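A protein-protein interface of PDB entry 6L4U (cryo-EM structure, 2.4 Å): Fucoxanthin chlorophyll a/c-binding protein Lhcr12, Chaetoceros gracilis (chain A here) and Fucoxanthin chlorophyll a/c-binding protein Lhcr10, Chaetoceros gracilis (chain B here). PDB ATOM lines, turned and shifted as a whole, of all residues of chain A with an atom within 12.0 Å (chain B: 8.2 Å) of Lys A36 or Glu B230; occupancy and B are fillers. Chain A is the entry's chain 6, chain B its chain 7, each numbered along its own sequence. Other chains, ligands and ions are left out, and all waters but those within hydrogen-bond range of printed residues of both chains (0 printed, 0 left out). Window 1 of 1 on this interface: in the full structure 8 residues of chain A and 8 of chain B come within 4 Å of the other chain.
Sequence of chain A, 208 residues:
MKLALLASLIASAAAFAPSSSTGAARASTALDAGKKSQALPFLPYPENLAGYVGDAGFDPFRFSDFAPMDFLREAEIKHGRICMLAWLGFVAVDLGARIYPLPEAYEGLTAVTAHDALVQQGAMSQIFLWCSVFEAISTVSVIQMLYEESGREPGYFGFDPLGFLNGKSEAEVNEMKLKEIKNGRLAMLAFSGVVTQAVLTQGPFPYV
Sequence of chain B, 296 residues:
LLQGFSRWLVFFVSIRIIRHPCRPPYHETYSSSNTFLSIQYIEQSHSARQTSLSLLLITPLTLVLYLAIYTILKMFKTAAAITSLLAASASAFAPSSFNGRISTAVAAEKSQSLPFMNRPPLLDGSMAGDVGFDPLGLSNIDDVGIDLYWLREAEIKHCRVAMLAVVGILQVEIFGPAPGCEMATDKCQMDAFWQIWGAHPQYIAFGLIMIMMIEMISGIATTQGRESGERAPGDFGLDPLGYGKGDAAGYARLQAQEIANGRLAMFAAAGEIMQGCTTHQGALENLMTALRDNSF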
ATOM      1  N   LYS A  35     -17.883  -2.628 -20.153  1.00  0.00           N
ATOM      2  CA  LYS A  35     -17.225  -2.347 -18.882  1.00  0.00           C
ATOM      3  C   LYS A  35     -17.120  -3.602 -18.036  1.00  0.00           C
ATOM      4  O   LYS A  35     -17.929  -4.518 -18.192  1.00  0.00           O
ATOM      5  CB  LYS A  35     -17.984  -1.267 -18.112  1.00  0.00           C
ATOM      6  CG  LYS A  35     -17.889   0.115 -18.727  1.00  0.00           C
ATOM      7  CD  LYS A  35     -18.791   1.097 -18.005  1.00  0.00           C
ATOM      8  CE  LYS A  35     -18.264   1.415 -16.619  1.00  0.00           C
ATOM      9  NZ  LYS A  35     -19.101   2.438 -15.935  1.00  0.00           N
ATOM     10  N   LYS A  36     -16.119  -3.619 -17.147  1.00  0.00           N
ATOM     11  CA  LYS A  36     -15.900  -4.670 -16.154  1.00  0.00           C
ATOM     12  C   LYS A  36     -15.709  -6.050 -16.770  1.00  0.00           C
ATOM     13  O   LYS A  36     -16.645  -6.857 -16.781  1.00  0.00           O
ATOM     14  CB  LYS A  36     -17.025  -4.693 -15.118  1.00  0.00           C
ATOM     15  CG  LYS A  36     -17.135  -3.416 -14.294  1.00  0.00           C
ATOM     16  CD  LYS A  36     -15.941  -3.220 -13.369  1.00  0.00           C
ATOM     17  CE  LYS A  36     -15.123  -1.991 -13.756  1.00  0.00           C
ATOM     18  NZ  LYS A  36     -13.963  -1.783 -12.847  1.00  0.00           N
ATOM     19  N   SER A  37     -14.542  -6.250 -17.392  1.00  0.00           N
ATOM     20  CA  SER A  37     -14.020  -7.557 -17.796  1.00  0.00           C
ATOM     21  C   SER A  37     -14.272  -8.642 -16.755  1.00  0.00           C
ATOM     22  O   SER A  37     -14.124  -8.418 -15.555  1.00  0.00           O
ATOM     23  CB  SER A  37     -12.519  -7.434 -18.045  1.00  0.00           C
ATOM     24  OG  SER A  37     -11.869  -8.677 -17.864  1.00  0.00           O
ATOM     25  N   GLN A  38     -14.657  -9.826 -17.232  1.00  0.00           N
ATOM     26  CA  GLN A  38     -15.139 -10.871 -16.334  1.00  0.00           C
ATOM     27  C   GLN A  38     -14.001 -11.534 -15.567  1.00  0.00           C
ATOM     28  O   GLN A  38     -14.110 -11.752 -14.356  1.00  0.00           O
ATOM     29  CB  GLN A  38     -15.926 -11.914 -17.122  1.00  0.00           C
ATOM     30  CG  GLN A  38     -16.396 -13.081 -16.288  1.00  0.00           C
ATOM     31  CD  GLN A  38     -16.905 -14.225 -17.122  1.00  0.00           C
ATOM     32  OE1 GLN A  38     -16.851 -14.184 -18.349  1.00  0.00           O
ATOM     33  NE2 GLN A  38     -17.409 -15.257 -16.462  1.00  0.00           N
ATOM     34  N   ALA A  39     -12.907 -11.868 -16.255  1.00  0.00           N
ATOM     35  CA  ALA A  39     -11.797 -12.565 -15.615  1.00  0.00           C
ATOM     36  C   ALA A  39     -11.064 -11.675 -14.627  1.00  0.00           C
ATOM     37  O   ALA A  39     -10.561 -12.159 -13.605  1.00  0.00           O
ATOM     38  CB  ALA A  39     -10.824 -13.074 -16.674  1.00  0.00           C
ATOM     39  N   LEU A  40     -10.998 -10.380 -14.916  1.00  0.00           N
ATOM     40  CA  LEU A  40     -10.334  -9.393 -14.076  1.00  0.00           C
ATOM     41  C   LEU A  40     -11.353  -8.309 -13.761  1.00  0.00           C
ATOM     42  O   LEU A  40     -11.384  -7.264 -14.422  1.00  0.00           O
ATOM     43  CB  LEU A  40      -9.110  -8.812 -14.780  1.00  0.00           C
ATOM     44  CG  LEU A  40      -8.091  -9.819 -15.305  1.00  0.00           C
ATOM     45  CD1 LEU A  40      -7.245  -9.206 -16.391  1.00  0.00           C
ATOM     46  CD2 LEU A  40      -7.220 -10.296 -14.184  1.00  0.00           C
ATOM     47  N   PRO A  41     -12.202  -8.518 -12.745  1.00  0.00           N
ATOM     48  CA  PRO A  41     -13.309  -7.578 -12.491  1.00  0.00           C
ATOM     49  C   PRO A  41     -12.880  -6.215 -11.977  1.00  0.00           C
ATOM     50  O   PRO A  41     -13.721  -5.314 -11.893  1.00  0.00           O
ATOM     51  CB  PRO A  41     -14.161  -8.316 -11.454  1.00  0.00           C
ATOM     52  CG  PRO A  41     -13.235  -9.259 -10.804  1.00  0.00           C
ATOM     53  CD  PRO A  41     -12.227  -9.666 -11.825  1.00  0.00           C
ATOM     54  N   PHE A  42     -11.610  -6.036 -11.641  1.00  0.00           N
ATOM     55  CA  PHE A  42     -11.046  -4.755 -11.259  1.00  0.00           C
ATOM     56  C   PHE A  42     -10.509  -3.979 -12.450  1.00  0.00           C
ATOM     57  O   PHE A  42      -9.887  -2.930 -12.260  1.00  0.00           O
ATOM     58  CB  PHE A  42      -9.930  -4.968 -10.231  1.00  0.00           C
ATOM     59  CG  PHE A  42      -9.011  -6.116 -10.554  1.00  0.00           C
ATOM     60  CD1 PHE A  42      -7.932  -5.936 -11.398  1.00  0.00           C
ATOM     61  CD2 PHE A  42      -9.213  -7.366  -9.994  1.00  0.00           C
ATOM     62  CE1 PHE A  42      -7.088  -6.980 -11.695  1.00  0.00           C
ATOM     63  CE2 PHE A  42      -8.373  -8.412 -10.289  1.00  0.00           C
ATOM     64  CZ  PHE A  42      -7.306  -8.217 -11.138  1.00  0.00           C
ATOM     65  N   LEU A  43     -10.733  -4.468 -13.665  1.00  0.00           N
ATOM     66  CA  LEU A  43     -10.208  -3.895 -14.890  1.00  0.00           C
ATOM     67  C   LEU A  43     -11.324  -3.700 -15.906  1.00  0.00           C
ATOM     68  O   LEU A  43     -12.277  -4.482 -15.939  1.00  0.00           O
ATOM     69  CB  LEU A  43      -9.126  -4.801 -15.487  1.00  0.00           C
ATOM     70  CG  LEU A  43      -7.694  -4.494 -15.063  1.00  0.00           C
ATOM     71  CD1 LEU A  43      -6.820  -5.695 -15.260  1.00  0.00           C
ATOM     72  CD2 LEU A  43      -7.159  -3.345 -15.870  1.00  0.00           C
ATOM     73  N   PRO A  44     -11.247  -2.662 -16.736  1.00  0.00           N
ATOM     74  CA  PRO A  44     -12.263  -2.475 -17.773  1.00  0.00           C
ATOM     75  C   PRO A  44     -12.117  -3.488 -18.896  1.00  0.00           C
ATOM     76  O   PRO A  44     -11.094  -4.155 -19.053  1.00  0.00           O
ATOM     77  CB  PRO A  44     -12.000  -1.053 -18.273  1.00  0.00           C
ATOM     78  CG  PRO A  44     -10.570  -0.827 -17.988  1.00  0.00           C
ATOM     79  CD  PRO A  44     -10.313  -1.526 -16.688  1.00  0.00           C
ATOM     80  N   TYR A  45     -13.168  -3.585 -19.684  1.00  0.00           N
ATOM     81  CA  TYR A  45     -13.262  -4.601 -20.722  1.00  0.00           C
ATOM     82  C   TYR A  45     -12.463  -4.188 -21.954  1.00  0.00           C
ATOM     83  O   TYR A  45     -12.655  -3.082 -22.465  1.00  0.00           O
ATOM     84  CB  TYR A  45     -14.718  -4.815 -21.096  1.00  0.00           C
ATOM     85  CG  TYR A  45     -14.958  -6.003 -21.980  1.00  0.00           C
ATOM     86  CD1 TYR A  45     -14.908  -7.292 -21.470  1.00  0.00           C
ATOM     87  CD2 TYR A  45     -15.240  -5.837 -23.328  1.00  0.00           C
ATOM     88  CE1 TYR A  45     -15.133  -8.381 -22.280  1.00  0.00           C
ATOM     89  CE2 TYR A  45     -15.464  -6.916 -24.144  1.00  0.00           C
ATOM     90  CZ  TYR A  45     -15.409  -8.184 -23.615  1.00  0.00           C
ATOM     91  OH  TYR A  45     -15.635  -9.262 -24.429  1.00  0.00           O
ATOM     92  N   PRO A  46     -11.562  -5.037 -22.453  1.00  0.00           N
ATOM     93  CA  PRO A  46     -10.928  -4.772 -23.755  1.00  0.00           C
ATOM     94  C   PRO A  46     -11.915  -5.048 -24.880  1.00  0.00           C
ATOM     95  O   PRO A  46     -12.288  -6.196 -25.129  1.00  0.00           O
ATOM     96  CB  PRO A  46      -9.740  -5.739 -23.780  1.00  0.00           C
ATOM     97  CG  PRO A  46     -10.074  -6.799 -22.803  1.00  0.00           C
ATOM     98  CD  PRO A  46     -11.027  -6.242 -21.798  1.00  0.00           C
ATOM     99  N   GLU A  47     -12.337  -3.986 -25.563  1.00  0.00           N
ATOM    100  CA  GLU A  47     -13.504  -4.053 -26.432  1.00  0.00           C
ATOM    101  C   GLU A  47     -13.251  -4.765 -27.755  1.00  0.00           C
ATOM    102  O   GLU A  47     -14.215  -5.078 -28.458  1.00  0.00           O
ATOM    103  CB  GLU A  47     -14.033  -2.644 -26.698  1.00  0.00           C
ATOM    104  CG  GLU A  47     -14.659  -1.986 -25.478  1.00  0.00           C
ATOM    105  CD  GLU A  47     -15.996  -2.600 -25.093  1.00  0.00           C
ATOM    106  OE1 GLU A  47     -16.345  -2.566 -23.893  1.00  0.00           O
ATOM    107  OE2 GLU A  47     -16.700  -3.113 -25.988  1.00  0.00           O
ATOM    108  N   ASN A  48     -11.998  -5.047 -28.108  1.00  0.00           N
ATOM    109  CA  ASN A  48     -11.724  -5.808 -29.319  1.00  0.00           C
ATOM    110  C   ASN A  48     -11.925  -7.307 -29.141  1.00  0.00           C
ATOM    111  O   ASN A  48     -11.801  -8.050 -30.118  1.00  0.00           O
ATOM    112  CB  ASN A  48     -10.299  -5.546 -29.803  1.00  0.00           C
ATOM    113  CG  ASN A  48     -10.119  -4.153 -30.350  1.00  0.00           C
ATOM    114  OD1 ASN A  48     -11.071  -3.523 -30.801  1.00  0.00           O
ATOM    115  ND2 ASN A  48      -8.889  -3.661 -30.319  1.00  0.00           N
ATOM    116  N   LEU A  49     -12.227  -7.767 -27.930  1.00  0.00           N
ATOM    117  CA  LEU A  49     -12.466  -9.183 -27.688  1.00  0.00           C
ATOM    118  C   LEU A  49     -13.888  -9.608 -28.011  1.00  0.00           C
ATOM    119  O   LEU A  49     -14.158 -10.811 -28.044  1.00  0.00           O
ATOM    120  CB  LEU A  49     -12.166  -9.531 -26.227  1.00  0.00           C
ATOM    121  CG  LEU A  49     -10.747  -9.328 -25.699  1.00  0.00           C
ATOM    122  CD1 LEU A  49     -10.532 -10.105 -24.415  1.00  0.00           C
ATOM    123  CD2 LEU A  49      -9.747  -9.751 -26.731  1.00  0.00           C
ATOM    124  N   ALA A  50     -14.789  -8.657 -28.242  1.00  0.00           N
ATOM    125  CA  ALA A  50     -16.206  -8.961 -28.397  1.00  0.00           C
ATOM    126  C   ALA A  50     -16.458  -9.666 -29.723  1.00  0.00           C
ATOM    127  O   ALA A  50     -16.036  -9.190 -30.781  1.00  0.00           O
ATOM    128  CB  ALA A  50     -17.025  -7.680 -28.305  1.00  0.00           C
ATOM    129  N   ASP A  55     -13.931 -15.908 -25.121  1.00  0.00           N
ATOM    130  CA  ASP A  55     -13.900 -14.597 -24.486  1.00  0.00           C
ATOM    131  C   ASP A  55     -14.178 -14.715 -22.997  1.00  0.00           C
ATOM    132  O   ASP A  55     -15.288 -15.064 -22.586  1.00  0.00           O
ATOM    133  CB  ASP A  55     -14.924 -13.688 -25.157  1.00  0.00           C
ATOM    134  CG  ASP A  55     -14.688 -12.234 -24.861  1.00  0.00           C
ATOM    135  OD1 ASP A  55     -13.622 -11.903 -24.306  1.00  0.00           O
ATOM    136  OD2 ASP A  55     -15.567 -11.416 -25.192  1.00  0.00           O
ATOM    137  N   ALA A  56     -13.169 -14.417 -22.187  1.00  0.00           N
ATOM    138  CA  ALA A  56     -13.336 -14.233 -20.755  1.00  0.00           C
ATOM    139  C   ALA A  56     -13.019 -12.809 -20.335  1.00  0.00           C
ATOM    140  O   ALA A  56     -12.943 -12.527 -19.138  1.00  0.00           O
ATOM    141  CB  ALA A  56     -12.456 -15.217 -19.987  1.00  0.00           C
ATOM    142  N   GLY A  57     -12.838 -11.904 -21.293  1.00  0.00           N
ATOM    143  CA  GLY A  57     -12.414 -10.558 -20.981  1.00  0.00           C
ATOM    144  C   GLY A  57     -10.993 -10.462 -20.492  1.00  0.00           C
ATOM    145  O   GLY A  57     -10.657  -9.523 -19.772  1.00  0.00           O
ATOM    146  N   PHE A  58     -10.146 -11.415 -20.859  1.00  0.00           N
ATOM    147  CA  PHE A  58      -8.797 -11.513 -20.317  1.00  0.00           C
ATOM    148  C   PHE A  58      -7.806 -11.051 -21.377  1.00  0.00           C
ATOM    149  O   PHE A  58      -7.272 -11.846 -22.147  1.00  0.00           O
ATOM    150  CB  PHE A  58      -8.511 -12.932 -19.856  1.00  0.00           C
ATOM    151  CG  PHE A  58      -7.173 -13.097 -19.221  1.00  0.00           C
ATOM    152  CD1 PHE A  58      -6.904 -12.523 -17.995  1.00  0.00           C
ATOM    153  CD2 PHE A  58      -6.180 -13.825 -19.850  1.00  0.00           C
ATOM    154  CE1 PHE A  58      -5.669 -12.672 -17.405  1.00  0.00           C
ATOM    155  CE2 PHE A  58      -4.945 -13.976 -19.263  1.00  0.00           C
ATOM    156  CZ  PHE A  58      -4.690 -13.398 -18.041  1.00  0.00           C
ATOM    157  N   ASP A  59      -7.567  -9.743 -21.419  1.00  0.00           N
ATOM    158  CA  ASP A  59      -6.426  -9.177 -22.141  1.00  0.00           C
ATOM    159  C   ASP A  59      -5.928  -7.961 -21.372  1.00  0.00           C
ATOM    160  O   ASP A  59      -6.176  -6.813 -21.758  1.00  0.00           O
ATOM    161  CB  ASP A  59      -6.814  -8.818 -23.575  1.00  0.00           C
ATOM    162  CG  ASP A  59      -5.624  -8.414 -24.426  1.00  0.00           C
ATOM    163  OD1 ASP A  59      -4.471  -8.666 -24.022  1.00  0.00           O
ATOM    164  OD2 ASP A  59      -5.842  -7.846 -25.513  1.00  0.00           O
ATOM    165  N   PRO A  60      -5.220  -8.178 -20.257  1.00  0.00           N
ATOM    166  CA  PRO A  60      -4.756  -7.029 -19.470  1.00  0.00           C
ATOM    167  C   PRO A  60      -3.620  -6.269 -20.121  1.00  0.00           C
ATOM    168  O   PRO A  60      -3.482  -5.065 -19.878  1.00  0.00           O
ATOM    169  CB  PRO A  60      -4.320  -7.668 -18.150  1.00  0.00           C
ATOM    170  CG  PRO A  60      -3.935  -9.033 -18.520  1.00  0.00           C
ATOM    171  CD  PRO A  60      -4.864  -9.452 -19.606  1.00  0.00           C
ATOM    172  N   ARG A  62      -3.360  -5.704 -23.278  1.00  0.00           N
ATOM    173  CA  ARG A  62      -3.968  -5.033 -24.435  1.00  0.00           C
ATOM    174  C   ARG A  62      -3.225  -5.338 -25.733  1.00  0.00           C
ATOM    175  O   ARG A  62      -2.887  -4.443 -26.509  1.00  0.00           O
ATOM    176  CB  ARG A  62      -4.085  -3.524 -24.206  1.00  0.00           C
ATOM    177  CG  ARG A  62      -5.115  -3.148 -23.163  1.00  0.00           C
ATOM    178  CD  ARG A  62      -6.453  -3.790 -23.461  1.00  0.00           C
ATOM    179  NE  ARG A  62      -7.454  -3.440 -22.462  1.00  0.00           N
ATOM    180  CZ  ARG A  62      -8.215  -2.354 -22.522  1.00  0.00           C
ATOM    181  NH1 ARG A  62      -8.093  -1.515 -23.537  1.00  0.00           N
ATOM    182  NH2 ARG A  62      -9.100  -2.112 -21.567  1.00  0.00           N
ATOM    183  N   TYR B 149      -3.975   8.731  -5.388  1.00  0.00           N
ATOM    184  CA  TYR B 149      -4.431   7.391  -5.749  1.00  0.00           C
ATOM    185  C   TYR B 149      -3.289   6.389  -5.701  1.00  0.00           C
ATOM    186  O   TYR B 149      -3.465   5.270  -5.210  1.00  0.00           O
ATOM    187  CB  TYR B 149      -5.060   7.407  -7.145  1.00  0.00           C
ATOM    188  CG  TYR B 149      -5.835   6.158  -7.531  1.00  0.00           C
ATOM    189  CD1 TYR B 149      -5.189   5.019  -8.012  1.00  0.00           C
ATOM    190  CD2 TYR B 149      -7.213   6.132  -7.456  1.00  0.00           C
ATOM    191  CE1 TYR B 149      -5.887   3.897  -8.360  1.00  0.00           C
ATOM    192  CE2 TYR B 149      -7.923   5.012  -7.820  1.00  0.00           C
ATOM    193  CZ  TYR B 149      -7.254   3.896  -8.267  1.00  0.00           C
ATOM    194  OH  TYR B 149      -7.953   2.772  -8.627  1.00  0.00           O
ATOM    195  N   ALA B 221      -4.269  -2.146 -13.533  1.00  0.00           N
ATOM    196  CA  ALA B 221      -5.527  -1.799 -12.882  1.00  0.00           C
ATOM    197  C   ALA B 221      -5.411  -0.528 -12.055  1.00  0.00           C
ATOM    198  O   ALA B 221      -6.406   0.181 -11.872  1.00  0.00           O
ATOM    199  CB  ALA B 221      -5.997  -2.952 -12.003  1.00  0.00           C
ATOM    200  N   GLN B 224      -5.136   2.360 -14.925  1.00  0.00           N
ATOM    201  CA  GLN B 224      -6.416   2.505 -15.604  1.00  0.00           C
ATOM    202  C   GLN B 224      -7.522   2.873 -14.628  1.00  0.00           C
ATOM    203  O   GLN B 224      -8.477   3.555 -15.011  1.00  0.00           O
ATOM    204  CB  GLN B 224      -6.765   1.226 -16.364  1.00  0.00           C
ATOM    205  CG  GLN B 224      -5.855   0.984 -17.558  1.00  0.00           C
ATOM    206  CD  GLN B 224      -6.265  -0.211 -18.393  1.00  0.00           C
ATOM    207  OE1 GLN B 224      -7.232  -0.899 -18.084  1.00  0.00           O
ATOM    208  NE2 GLN B 224      -5.523  -0.463 -19.465  1.00  0.00           N
ATOM    209  N   GLY B 225      -7.409   2.451 -13.367  1.00  0.00           N
ATOM    210  CA  GLY B 225      -8.370   2.863 -12.362  1.00  0.00           C
ATOM    211  C   GLY B 225      -8.215   4.302 -11.932  1.00  0.00           C
ATOM    212  O   GLY B 225      -9.163   4.890 -11.403  1.00  0.00           O
ATOM    213  N   ARG B 226      -7.042   4.883 -12.153  1.00  0.00           N
ATOM    214  CA  ARG B 226      -6.785   6.284 -11.867  1.00  0.00           C
ATOM    215  C   ARG B 226      -7.268   7.188 -12.994  1.00  0.00           C
ATOM    216  O   ARG B 226      -7.871   8.233 -12.731  1.00  0.00           O
ATOM    217  CB  ARG B 226      -5.290   6.485 -11.615  1.00  0.00           C
ATOM    218  CG  ARG B 226      -4.810   7.907 -11.664  1.00  0.00           C
ATOM    219  CD  ARG B 226      -3.444   8.011 -11.045  1.00  0.00           C
ATOM    220  NE  ARG B 226      -2.429   7.288 -11.801  1.00  0.00           N
ATOM    221  CZ  ARG B 226      -1.138   7.279 -11.492  1.00  0.00           C
ATOM    222  NH1 ARG B 226      -0.702   7.948 -10.436  1.00  0.00           N
ATOM    223  NH2 ARG B 226      -0.282   6.596 -12.235  1.00  0.00           N
ATOM    224  N   GLU B 227      -7.023   6.792 -14.248  1.00  0.00           N
ATOM    225  CA  GLU B 227      -7.481   7.575 -15.392  1.00  0.00           C
ATOM    226  C   GLU B 227      -8.998   7.577 -15.498  1.00  0.00           C
ATOM    227  O   GLU B 227      -9.594   8.607 -15.828  1.00  0.00           O
ATOM    228  CB  GLU B 227      -6.868   7.030 -16.680  1.00  0.00           C
ATOM    229  CG  GLU B 227      -5.375   7.267 -16.817  1.00  0.00           C
ATOM    230  CD  GLU B 227      -4.793   6.617 -18.059  1.00  0.00           C
ATOM    231  OE1 GLU B 227      -5.521   5.847 -18.723  1.00  0.00           O
ATOM    232  OE2 GLU B 227      -3.610   6.875 -18.370  1.00  0.00           O
ATOM    233  N   SER B 228      -9.633   6.450 -15.214  1.00  0.00           N
ATOM    234  CA  SER B 228     -11.078   6.380 -15.106  1.00  0.00           C
ATOM    235  C   SER B 228     -11.469   6.637 -13.652  1.00  0.00           C
ATOM    236  O   SER B 228     -10.684   7.159 -12.857  1.00  0.00           O
ATOM    237  CB  SER B 228     -11.581   5.035 -15.615  1.00  0.00           C
ATOM    238  OG  SER B 228     -11.172   3.981 -14.765  1.00  0.00           O
ATOM    239  N   GLY B 229     -12.693   6.284 -13.284  1.00  0.00           N
ATOM    240  CA  GLY B 229     -13.104   6.428 -11.905  1.00  0.00           C
ATOM    241  C   GLY B 229     -13.874   5.235 -11.383  1.00  0.00           C
ATOM    242  O   GLY B 229     -14.608   5.351 -10.399  1.00  0.00           O
ATOM    243  N   GLU B 230     -13.720   4.079 -12.028  1.00  0.00           N
ATOM    244  CA  GLU B 230     -14.479   2.892 -11.670  1.00  0.00           C
ATOM    245  C   GLU B 230     -13.724   1.946 -10.747  1.00  0.00           C
ATOM    246  O   GLU B 230     -14.142   0.795 -10.584  1.00  0.00           O
ATOM    247  CB  GLU B 230     -14.924   2.137 -12.926  1.00  0.00           C
ATOM    248  CG  GLU B 230     -16.138   2.736 -13.627  1.00  0.00           C
ATOM    249  CD  GLU B 230     -15.781   3.775 -14.666  1.00  0.00           C
ATOM    250  OE1 GLU B 230     -14.599   4.158 -14.747  1.00  0.00           O
ATOM    251  OE2 GLU B 230     -16.692   4.214 -15.400  1.00  0.00           O
ATOM    252  N   ARG B 231     -12.639   2.396 -10.126  1.00  0.00           N
ATOM    253  CA  ARG B 231     -11.907   1.523  -9.216  1.00  0.00           C
ATOM    254  C   ARG B 231     -11.371   2.335  -8.052  1.00  0.00           C
ATOM    255  O   ARG B 231     -10.621   3.291  -8.256  1.00  0.00           O
ATOM    256  CB  ARG B 231     -10.766   0.807  -9.933  1.00  0.00           C
ATOM    257  CG  ARG B 231     -10.100  -0.237  -9.076  1.00  0.00           C
ATOM    258  CD  ARG B 231      -8.729  -0.578  -9.589  1.00  0.00           C
ATOM    259  NE  ARG B 231      -8.065  -1.539  -8.719  1.00  0.00           N
ATOM    260  CZ  ARG B 231      -7.033  -1.246  -7.938  1.00  0.00           C
ATOM    261  NH1 ARG B 231      -6.493  -2.183  -7.177  1.00  0.00           N
ATOM    262  NH2 ARG B 231      -6.542  -0.018  -7.921  1.00  0.00           N
ATOM    263  N   ALA B 232     -11.767   1.958  -6.842  1.00  0.00           N
ATOM    264  CA  ALA B 232     -11.156   2.511  -5.649  1.00  0.00           C
ATOM    265  C   ALA B 232      -9.721   2.001  -5.532  1.00  0.00           C
ATOM    266  O   ALA B 232      -9.399   0.931  -6.052  1.00  0.00           O
ATOM    267  CB  ALA B 232     -11.963   2.120  -4.414  1.00  0.00           C
ATOM    268  N   PRO B 233      -8.828   2.760  -4.894  1.00  0.00           N
ATOM    269  CA  PRO B 233      -7.445   2.282  -4.740  1.00  0.00           C
ATOM    270  C   PRO B 233      -7.377   1.087  -3.800  1.00  0.00           C
ATOM    271  O   PRO B 233      -7.999   1.077  -2.737  1.00  0.00           O
ATOM    272  CB  PRO B 233      -6.701   3.497  -4.173  1.00  0.00           C
ATOM    273  CG  PRO B 233      -7.742   4.441  -3.735  1.00  0.00           C
ATOM    274  CD  PRO B 233      -8.963   4.178  -4.522  1.00  0.00           C
ATOM    275  N   ASP B 235      -8.704  -1.759  -4.487  1.00  0.00           N
ATOM    276  CA  ASP B 235      -9.912  -2.551  -4.659  1.00  0.00           C
ATOM    277  C   ASP B 235      -9.708  -3.526  -5.810  1.00  0.00           C
ATOM    278  O   ASP B 235      -9.346  -3.124  -6.918  1.00  0.00           O
ATOM    279  CB  ASP B 235     -11.111  -1.642  -4.922  1.00  0.00           C
ATOM    280  CG  ASP B 235     -12.427  -2.385  -4.909  1.00  0.00           C
ATOM    281  OD1 ASP B 235     -12.463  -3.547  -4.460  1.00  0.00           O
ATOM    282  OD2 ASP B 235     -13.435  -1.799  -5.351  1.00  0.00           O
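O of Glu B230 lies within hydrogen-bond range of NZ of Lys A36 (3.4 Å).
The side-chain carboxylate (OE2) of Glu B230 lies within salt-bridge range of the side-chain amino group (NZ) of Lys A35 (3.0 Å).
O of Gln B224 lies within hydrogen-bond range of OG of Ser B228 (2.7 Å).
The backbone carbonyl oxygen of Leu A43 sits at hydrogen-bond distance from the backbone NH of Ser A37.
OG of Ser B228 lies close to OE1 of Glu B230 (3.4 Å).
NE of Arg B231 sits at hydrogen-bond distance from O of Asp B235.
OH of Tyr B149 is in hydrogen-bond range of O of Arg B231 (2.7 Å).
CB of Ala B221 touches CD1 of Phe A42, at 3.6 Å.
O of Phe A42 touches CD of Arg B231 (3.7 Å).
CB of Phe A42 touches O of Asp B235, 3.8 Å away.
CD2 of Leu A43 touches CA of Ala B221 (3.7 Å).
Leu A43 touches Gln B224.
CG of Pro A44 touches OE1 of Gln B224 (3.3 Å).
Lys A36 touches just one residue of chain B: Glu B230.
Glu B230 touches two residues of chain A.
Gly B225 touches none of the printed residues of chain A.
No residue of chain A comes within 4 Å of Ser B228.
No residue of chain A comes within 4 Å of Gly B229.
No residue of chain A comes within 4 Å of Ala B232.
Of the printed residues of chain B, Lys A35 touches Glu B230.
Of the printed residues of chain B, Phe A42 touches Ala B221 (3.6 Å), Arg B231 (3.7 Å) and Asp B235 (3.8 Å).
Of the printed residues of chain A, Gln B224 touches Leu A43 and Pro A44.
The nearest residue of chain B that does not touch Lys A36 is Arg B231 (5.0 Å).
Of the 13 printed residues of chain B, 5 touch a printed residue of chain A.
Printed residues of chain B that touch a printed residue of chain A: Ala B221, Gln B224, Glu B230, Arg B231 and Asp B235.
Hydrophobic or aromatic side chains of chain B within 4 Å of the printed part of chain A: Ala B221.
Of the 23 printed residues of chain A, 5 touch a printed residue of chain B.
Hydrophobic or aromatic side chains of chain A within 4 Å of the printed part of chain B: Phe A42, Leu A43 and Pro A44.
Among the printed residues, Asp or Glu carboxylates within 4 Å of a Lys or Arg side-chain nitrogen of the other chain: Lys A35 with Glu B230 (3.0 Å).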
